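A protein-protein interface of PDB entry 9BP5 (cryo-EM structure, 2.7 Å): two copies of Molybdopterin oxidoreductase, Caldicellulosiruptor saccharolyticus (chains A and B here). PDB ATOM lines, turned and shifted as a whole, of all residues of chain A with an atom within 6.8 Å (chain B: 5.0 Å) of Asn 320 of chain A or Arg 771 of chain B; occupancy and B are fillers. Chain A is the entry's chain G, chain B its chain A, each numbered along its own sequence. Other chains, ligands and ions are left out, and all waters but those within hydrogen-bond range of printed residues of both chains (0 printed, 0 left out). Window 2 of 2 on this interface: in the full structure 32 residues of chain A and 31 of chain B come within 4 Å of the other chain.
Printed residues of chain B within 4 Å of Gln 317 of chain A: Gln 768. Of the printed residues of chain B, Asn 320 of chain A touches Arg 771 (3.3 Å). Of the printed residues of chain B, Leu 321 of chain A touches Ala 772 (2.7 Å) and Ser 773 (3.8 Å). Printed residues of chain A within 4 Å of Gln 768 of chain B: Gln 317 (2.9 Å). Of the printed residues of chain A, Ala 769 of chain B touches Leu 344. Of chain A, only Pro 318, Val 319 and Asn 320 come within 4 Å of Arg 771 of chain B. Of the printed residues of chain A, Ser 773 of chain B touches Leu 321 (3.8 Å) and Leu 344 (3.7 Å). The nearest residue of chain A that does not touch Arg 771 of chain B is Leu 321 of chain A (5.9 Å). The nearest printed residue of chain A that does not touch Ala 772 of chain B is Leu 344 of chain A (4.3 Å).
Among the printed residues, pairs that only touch across the chains: Val 319 of chain A with Ala 772 of chain B (3.2 Å), Pro 318 of chain A with Arg 771 of chain B (3.6 Å), Leu 344 of chain A with Ser 773 of chain B (3.7 Å), Val 319 of chain A with Arg 771 of chain B (3.8 Å) and Leu 321 of chain A with Ser 773 of chain B (3.8 Å).
The side-chain amide nitrogen of Gln 768 of chain B lies within hydrogen-bond range of the backbone carbonyl oxygen of Gln 317 of chain A, at 2.9 Å. The side-chain amide nitrogen (ND2) of Asn 320 of chain A lies close to the guanidinium group (NH2) of Arg 771 of chain B (3.3 Å). O of Ala 772 of chain B sits close to O of Leu 321 of chain A, at 2.7 Å. The backbone carbonyl oxygen (O) of Leu 344 of chain A sits close to the backbone carbonyl oxygen (O) of Ala 769 of chain B.
No position is printed for both chains. Of the 9 pairs that touch across the chains among the printed residues, none has its exchanged pair printed and touching as well.
The backbone carbonyl oxygen (O) of Ala 769 of chain B is in hydrogen-bond range of the side-chain hydroxyl (OG) of Ser 773 of chain B (2.6 Å). OD2 of Asp 803 of chain B lies within salt-bridge range of NE of Arg 771 of chain B.
Of the 14 printed residues of chain B, 5 touch a printed residue of chain A. Printed residues of chain B that touch a printed residue of chain A: Gln 768, Ala 769, Arg 771, Ala 772 and Ser 773. Hydrophobic or aromatic side chains of chain B that line the printed part of chain A: Ala 769 and Ala 772. Hydrophobic or aromatic side chains of chain A within 4 Å of the printed part of chain B: Pro 318, Val 319 and Leu 344. Among the printed residues, 9 pairs touch across the chains.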
ATOM      1  N   GLU A 301       0.639   4.986 -29.838  1.00  0.00           N
ATOM      2  CA  GLU A 301       0.933   6.349 -29.414  1.00  0.00           C
ATOM      3  C   GLU A 301       1.714   6.276 -28.109  1.00  0.00           C
ATOM      4  O   GLU A 301       1.150   5.975 -27.054  1.00  0.00           O
ATOM      5  CB  GLU A 301      -0.353   7.155 -29.252  1.00  0.00           C
ATOM      6  CG  GLU A 301      -0.206   8.637 -29.553  1.00  0.00           C
ATOM      7  CD  GLU A 301       0.297   9.428 -28.361  1.00  0.00           C
ATOM      8  OE1 GLU A 301       0.171   8.936 -27.220  1.00  0.00           O
ATOM      9  OE2 GLU A 301       0.820  10.544 -28.567  1.00  0.00           O
ATOM     10  N   GLY A 302       3.015   6.542 -28.183  1.00  0.00           N
ATOM     11  CA  GLY A 302       3.865   6.426 -27.018  1.00  0.00           C
ATOM     12  C   GLY A 302       5.115   5.619 -27.290  1.00  0.00           C
ATOM     13  O   GLY A 302       5.938   5.417 -26.395  1.00  0.00           O
ATOM     14  N   ILE A 304       8.461   5.694 -29.736  1.00  0.00           N
ATOM     15  CA  ILE A 304       9.222   6.632 -30.548  1.00  0.00           C
ATOM     16  C   ILE A 304      10.618   6.066 -30.758  1.00  0.00           C
ATOM     17  O   ILE A 304      11.132   5.308 -29.930  1.00  0.00           O
ATOM     18  CB  ILE A 304       9.263   8.041 -29.901  1.00  0.00           C
ATOM     19  CG1 ILE A 304       9.707   9.095 -30.916  1.00  0.00           C
ATOM     20  CG2 ILE A 304      10.148   8.053 -28.670  1.00  0.00           C
ATOM     21  CD1 ILE A 304       9.702  10.503 -30.378  1.00  0.00           C
ATOM     22  N   PHE A 309      13.640  10.700 -30.975  1.00  0.00           N
ATOM     23  CA  PHE A 309      13.457  11.308 -29.662  1.00  0.00           C
ATOM     24  C   PHE A 309      14.618  12.232 -29.312  1.00  0.00           C
ATOM     25  O   PHE A 309      14.410  13.351 -28.830  1.00  0.00           O
ATOM     26  CB  PHE A 309      13.296  10.206 -28.616  1.00  0.00           C
ATOM     27  CG  PHE A 309      13.524  10.653 -27.204  1.00  0.00           C
ATOM     28  CD1 PHE A 309      12.582  11.417 -26.542  1.00  0.00           C
ATOM     29  CD2 PHE A 309      14.670  10.283 -26.529  1.00  0.00           C
ATOM     30  CE1 PHE A 309      12.791  11.817 -25.241  1.00  0.00           C
ATOM     31  CE2 PHE A 309      14.883  10.683 -25.227  1.00  0.00           C
ATOM     32  CZ  PHE A 309      13.941  11.449 -24.583  1.00  0.00           C
ATOM     33  N   GLN A 317      12.122  20.645 -29.131  1.00  0.00           N
ATOM     34  CA  GLN A 317      10.737  20.404 -29.494  1.00  0.00           C
ATOM     35  C   GLN A 317      10.052  19.549 -28.434  1.00  0.00           C
ATOM     36  O   GLN A 317      10.705  18.747 -27.761  1.00  0.00           O
ATOM     37  CB  GLN A 317      10.657  19.712 -30.847  1.00  0.00           C
ATOM     38  CG  GLN A 317      11.157  20.570 -31.987  1.00  0.00           C
ATOM     39  CD  GLN A 317      11.262  19.810 -33.285  1.00  0.00           C
ATOM     40  OE1 GLN A 317      11.246  18.582 -33.301  1.00  0.00           O
ATOM     41  NE2 GLN A 317      11.376  20.537 -34.386  1.00  0.00           N
ATOM     42  N   PRO A 318       8.743  19.717 -28.248  1.00  0.00           N
ATOM     43  CA  PRO A 318       8.050  18.968 -27.194  1.00  0.00           C
ATOM     44  C   PRO A 318       8.068  17.468 -27.454  1.00  0.00           C
ATOM     45  O   PRO A 318       7.903  17.008 -28.584  1.00  0.00           O
ATOM     46  CB  PRO A 318       6.626  19.530 -27.240  1.00  0.00           C
ATOM     47  CG  PRO A 318       6.767  20.863 -27.884  1.00  0.00           C
ATOM     48  CD  PRO A 318       7.849  20.687 -28.898  1.00  0.00           C
ATOM     49  N   VAL A 319       8.261  16.709 -26.381  1.00  0.00           N
ATOM     50  CA  VAL A 319       8.225  15.254 -26.417  1.00  0.00           C
ATOM     51  C   VAL A 319       7.216  14.794 -25.379  1.00  0.00           C
ATOM     52  O   VAL A 319       7.196  15.308 -24.257  1.00  0.00           O
ATOM     53  CB  VAL A 319       9.608  14.630 -26.148  1.00  0.00           C
ATOM     54  CG1 VAL A 319      10.460  14.681 -27.396  1.00  0.00           C
ATOM     55  CG2 VAL A 319      10.305  15.337 -25.003  1.00  0.00           C
ATOM     56  N   ASN A 320       6.364  13.850 -25.759  1.00  0.00           N
ATOM     57  CA  ASN A 320       5.338  13.338 -24.855  1.00  0.00           C
ATOM     58  C   ASN A 320       5.883  12.212 -23.985  1.00  0.00           C
ATOM     59  O   ASN A 320       5.357  11.102 -23.953  1.00  0.00           O
ATOM     60  CB  ASN A 320       4.126  12.885 -25.655  1.00  0.00           C
ATOM     61  CG  ASN A 320       3.261  14.043 -26.101  1.00  0.00           C
ATOM     62  OD1 ASN A 320       3.030  14.238 -27.293  1.00  0.00           O
ATOM     63  ND2 ASN A 320       2.783  14.824 -25.141  1.00  0.00           N
ATOM     64  N   LEU A 321       6.966  12.503 -23.277  1.00  0.00           N
ATOM     65  CA  LEU A 321       7.592  11.535 -22.394  1.00  0.00           C
ATOM     66  C   LEU A 321       6.770  11.391 -21.122  1.00  0.00           C
ATOM     67  O   LEU A 321       6.468  12.383 -20.455  1.00  0.00           O
ATOM     68  CB  LEU A 321       9.016  11.974 -22.063  1.00  0.00           C
ATOM     69  CG  LEU A 321       9.961  10.941 -21.462  1.00  0.00           C
ATOM     70  CD1 LEU A 321      10.738  10.253 -22.561  1.00  0.00           C
ATOM     71  CD2 LEU A 321      10.896  11.612 -20.482  1.00  0.00           C
ATOM     72  N   GLY A 322       6.415  10.160 -20.780  1.00  0.00           N
ATOM     73  CA  GLY A 322       5.579   9.939 -19.619  1.00  0.00           C
ATOM     74  C   GLY A 322       6.346   9.963 -18.317  1.00  0.00           C
ATOM     75  O   GLY A 322       7.233  10.799 -18.124  1.00  0.00           O
ATOM     76  N   LEU A 344      14.903  14.684 -18.308  1.00  0.00           N
ATOM     77  CA  LEU A 344      13.646  15.305 -18.697  1.00  0.00           C
ATOM     78  C   LEU A 344      12.547  15.091 -17.666  1.00  0.00           C
ATOM     79  O   LEU A 344      11.397  15.455 -17.920  1.00  0.00           O
ATOM     80  CB  LEU A 344      13.193  14.778 -20.061  1.00  0.00           C
ATOM     81  CG  LEU A 344      13.900  15.347 -21.293  1.00  0.00           C
ATOM     82  CD1 LEU A 344      13.148  14.977 -22.547  1.00  0.00           C
ATOM     83  CD2 LEU A 344      14.056  16.848 -21.197  1.00  0.00           C
ATOM     84  N   ASP A 427       4.733   4.230 -19.603  1.00  0.00           N
ATOM     85  CA  ASP A 427       4.024   5.298 -20.290  1.00  0.00           C
ATOM     86  C   ASP A 427       4.591   5.566 -21.674  1.00  0.00           C
ATOM     87  O   ASP A 427       3.873   6.091 -22.531  1.00  0.00           O
ATOM     88  CB  ASP A 427       4.068   6.588 -19.468  1.00  0.00           C
ATOM     89  CG  ASP A 427       3.494   6.417 -18.080  1.00  0.00           C
ATOM     90  OD1 ASP A 427       3.315   5.262 -17.643  1.00  0.00           O
ATOM     91  OD2 ASP A 427       3.219   7.442 -17.424  1.00  0.00           O
ATOM     92  N   THR A 428       5.858   5.231 -21.908  1.00  0.00           N
ATOM     93  CA  THR A 428       6.463   5.429 -23.215  1.00  0.00           C
ATOM     94  C   THR A 428       7.561   4.399 -23.434  1.00  0.00           C
ATOM     95  O   THR A 428       8.214   3.952 -22.486  1.00  0.00           O
ATOM     96  CB  THR A 428       7.020   6.851 -23.369  1.00  0.00           C
ATOM     97  OG1 THR A 428       7.657   6.990 -24.644  1.00  0.00           O
ATOM     98  CG2 THR A 428       8.013   7.155 -22.278  1.00  0.00           C
ATOM     99  N   LEU B 767      12.316  24.207 -19.061  1.00  0.00           N
ATOM    100  CA  LEU B 767      10.957  24.335 -19.573  1.00  0.00           C
ATOM    101  C   LEU B 767      10.567  23.127 -20.414  1.00  0.00           C
ATOM    102  O   LEU B 767       9.438  22.628 -20.313  1.00  0.00           O
ATOM    103  CB  LEU B 767      10.820  25.624 -20.377  1.00  0.00           C
ATOM    104  CG  LEU B 767      10.996  26.928 -19.601  1.00  0.00           C
ATOM    105  CD1 LEU B 767      10.810  28.114 -20.521  1.00  0.00           C
ATOM    106  CD2 LEU B 767      10.038  26.999 -18.430  1.00  0.00           C
ATOM    107  N   GLN B 768      11.487  22.635 -21.248  1.00  0.00           N
ATOM    108  CA  GLN B 768      11.184  21.463 -22.060  1.00  0.00           C
ATOM    109  C   GLN B 768      10.973  20.228 -21.197  1.00  0.00           C
ATOM    110  O   GLN B 768      10.114  19.398 -21.502  1.00  0.00           O
ATOM    111  CB  GLN B 768      12.295  21.221 -23.077  1.00  0.00           C
ATOM    112  CG  GLN B 768      11.901  20.230 -24.156  1.00  0.00           C
ATOM    113  CD  GLN B 768      13.089  19.550 -24.795  1.00  0.00           C
ATOM    114  OE1 GLN B 768      14.235  19.817 -24.445  1.00  0.00           O
ATOM    115  NE2 GLN B 768      12.818  18.656 -25.732  1.00  0.00           N
ATOM    116  N   ALA B 769      11.752  20.078 -20.125  1.00  0.00           N
ATOM    117  CA  ALA B 769      11.562  18.950 -19.223  1.00  0.00           C
ATOM    118  C   ALA B 769      10.206  19.013 -18.538  1.00  0.00           C
ATOM    119  O   ALA B 769       9.533  17.986 -18.384  1.00  0.00           O
ATOM    120  CB  ALA B 769      12.682  18.914 -18.186  1.00  0.00           C
ATOM    121  N   ILE B 770       9.789  20.208 -18.115  1.00  0.00           N
ATOM    122  CA  ILE B 770       8.470  20.347 -17.501  1.00  0.00           C
ATOM    123  C   ILE B 770       7.378  19.986 -18.502  1.00  0.00           C
ATOM    124  O   ILE B 770       6.444  19.240 -18.186  1.00  0.00           O
ATOM    125  CB  ILE B 770       8.278  21.770 -16.946  1.00  0.00           C
ATOM    126  CG1 ILE B 770       9.073  21.945 -15.652  1.00  0.00           C
ATOM    127  CG2 ILE B 770       6.806  22.053 -16.712  1.00  0.00           C
ATOM    128  CD1 ILE B 770       8.478  21.236 -14.468  1.00  0.00           C
ATOM    129  N   ARG B 771       7.491  20.496 -19.731  1.00  0.00           N
ATOM    130  CA  ARG B 771       6.486  20.199 -20.746  1.00  0.00           C
ATOM    131  C   ARG B 771       6.440  18.711 -21.060  1.00  0.00           C
ATOM    132  O   ARG B 771       5.360  18.139 -21.236  1.00  0.00           O
ATOM    133  CB  ARG B 771       6.762  21.008 -22.013  1.00  0.00           C
ATOM    134  CG  ARG B 771       6.245  20.385 -23.296  1.00  0.00           C
ATOM    135  CD  ARG B 771       4.736  20.509 -23.409  1.00  0.00           C
ATOM    136  NE  ARG B 771       4.199  19.808 -24.570  1.00  0.00           N
ATOM    137  CZ  ARG B 771       3.994  18.499 -24.633  1.00  0.00           C
ATOM    138  NH1 ARG B 771       4.286  17.704 -23.619  1.00  0.00           N
ATOM    139  NH2 ARG B 771       3.487  17.976 -25.744  1.00  0.00           N
ATOM    140  N   ALA B 772       7.604  18.064 -21.133  1.00  0.00           N
ATOM    141  CA  ALA B 772       7.641  16.634 -21.409  1.00  0.00           C
ATOM    142  C   ALA B 772       6.985  15.841 -20.290  1.00  0.00           C
ATOM    143  O   ALA B 772       6.068  15.050 -20.531  1.00  0.00           O
ATOM    144  CB  ALA B 772       9.083  16.178 -21.615  1.00  0.00           C
ATOM    145  N   SER B 773       7.412  16.067 -19.050  1.00  0.00           N
ATOM    146  CA  SER B 773       6.927  15.258 -17.942  1.00  0.00           C
ATOM    147  C   SER B 773       5.513  15.612 -17.501  1.00  0.00           C
ATOM    148  O   SER B 773       4.920  14.843 -16.738  1.00  0.00           O
ATOM    149  CB  SER B 773       7.878  15.375 -16.751  1.00  0.00           C
ATOM    150  OG  SER B 773       8.240  16.723 -16.512  1.00  0.00           O
ATOM    151  N   TYR B 774       4.948  16.736 -17.952  1.00  0.00           N
ATOM    152  CA  TYR B 774       3.622  17.137 -17.501  1.00  0.00           C
ATOM    153  C   TYR B 774       2.646  17.509 -18.608  1.00  0.00           C
ATOM    154  O   TYR B 774       1.457  17.660 -18.318  1.00  0.00           O
ATOM    155  CB  TYR B 774       3.729  18.308 -16.517  1.00  0.00           C
ATOM    156  CG  TYR B 774       4.347  17.906 -15.204  1.00  0.00           C
ATOM    157  CD1 TYR B 774       3.664  17.086 -14.322  1.00  0.00           C
ATOM    158  CD2 TYR B 774       5.622  18.326 -14.857  1.00  0.00           C
ATOM    159  CE1 TYR B 774       4.226  16.706 -13.127  1.00  0.00           C
ATOM    160  CE2 TYR B 774       6.192  17.951 -13.663  1.00  0.00           C
ATOM    161  CZ  TYR B 774       5.489  17.140 -12.803  1.00  0.00           C
ATOM    162  OH  TYR B 774       6.050  16.759 -11.609  1.00  0.00           O
ATOM    163  N   GLY B 775       3.090  17.661 -19.846  1.00  0.00           N
ATOM    164  CA  GLY B 775       2.171  17.841 -20.949  1.00  0.00           C
ATOM    165  C   GLY B 775       1.843  19.284 -21.264  1.00  0.00           C
ATOM    166  O   GLY B 775       2.491  20.235 -20.816  1.00  0.00           O
ATOM    167  N   LYS B 776       0.791  19.437 -22.062  1.00  0.00           N
ATOM    168  CA  LYS B 776       0.362  20.743 -22.540  1.00  0.00           C
ATOM    169  C   LYS B 776      -0.140  21.614 -21.396  1.00  0.00           C
ATOM    170  O   LYS B 776      -0.675  21.123 -20.399  1.00  0.00           O
ATOM    171  CB  LYS B 776      -0.748  20.595 -23.576  1.00  0.00           C
ATOM    172  CG  LYS B 776      -0.416  19.722 -24.763  1.00  0.00           C
ATOM    173  CD  LYS B 776      -0.922  20.356 -26.047  1.00  0.00           C
ATOM    174  CE  LYS B 776      -0.237  19.778 -27.265  1.00  0.00           C
ATOM    175  NZ  LYS B 776      -0.703  18.396 -27.560  1.00  0.00           N
ATOM    176  N   SER B 778       1.276  23.286 -19.074  1.00  0.00           N
ATOM    177  CA  SER B 778       1.895  23.062 -17.778  1.00  0.00           C
ATOM    178  C   SER B 778       2.871  24.158 -17.384  1.00  0.00           C
ATOM    179  O   SER B 778       3.381  24.131 -16.261  1.00  0.00           O
ATOM    180  CB  SER B 778       2.618  21.709 -17.764  1.00  0.00           C
ATOM    181  OG  SER B 778       3.200  21.434 -19.025  1.00  0.00           O
ATOM    182  N   ILE B 779       3.140  25.112 -18.268  1.00  0.00           N
ATOM    183  CA  ILE B 779       4.037  26.228 -17.997  1.00  0.00           C
ATOM    184  C   ILE B 779       3.235  27.514 -18.118  1.00  0.00           C
ATOM    185  O   ILE B 779       2.531  27.720 -19.112  1.00  0.00           O
ATOM    186  CB  ILE B 779       5.238  26.251 -18.960  1.00  0.00           C
ATOM    187  CG1 ILE B 779       6.067  24.976 -18.827  1.00  0.00           C
ATOM    188  CG2 ILE B 779       6.102  27.472 -18.709  1.00  0.00           C
ATOM    189  CD1 ILE B 779       6.589  24.463 -20.139  1.00  0.00           C
ATOM    190  N   LEU B 802       6.119  26.468 -26.624  1.00  0.00           N
ATOM    191  CA  LEU B 802       6.219  25.677 -25.406  1.00  0.00           C
ATOM    192  C   LEU B 802       4.965  24.870 -25.126  1.00  0.00           C
ATOM    193  O   LEU B 802       4.902  24.196 -24.094  1.00  0.00           O
ATOM    194  CB  LEU B 802       6.521  26.582 -24.211  1.00  0.00           C
ATOM    195  CG  LEU B 802       8.000  26.819 -23.926  1.00  0.00           C
ATOM    196  CD1 LEU B 802       8.192  28.095 -23.139  1.00  0.00           C
ATOM    197  CD2 LEU B 802       8.579  25.636 -23.185  1.00  0.00           C
ATOM    198  N   ASP B 803       3.968  24.939 -26.008  1.00  0.00           N
ATOM    199  CA  ASP B 803       2.742  24.151 -25.895  1.00  0.00           C
ATOM    200  C   ASP B 803       1.930  24.555 -24.668  1.00  0.00           C
ATOM    201  O   ASP B 803       1.435  23.709 -23.924  1.00  0.00           O
ATOM    202  CB  ASP B 803       3.055  22.653 -25.872  1.00  0.00           C
ATOM    203  CG  ASP B 803       2.635  21.951 -27.139  1.00  0.00           C
ATOM    204  OD1 ASP B 803       2.243  22.642 -28.102  1.00  0.00           O
ATOM    205  OD2 ASP B 803       2.722  20.708 -27.181  1.00  0.00           O
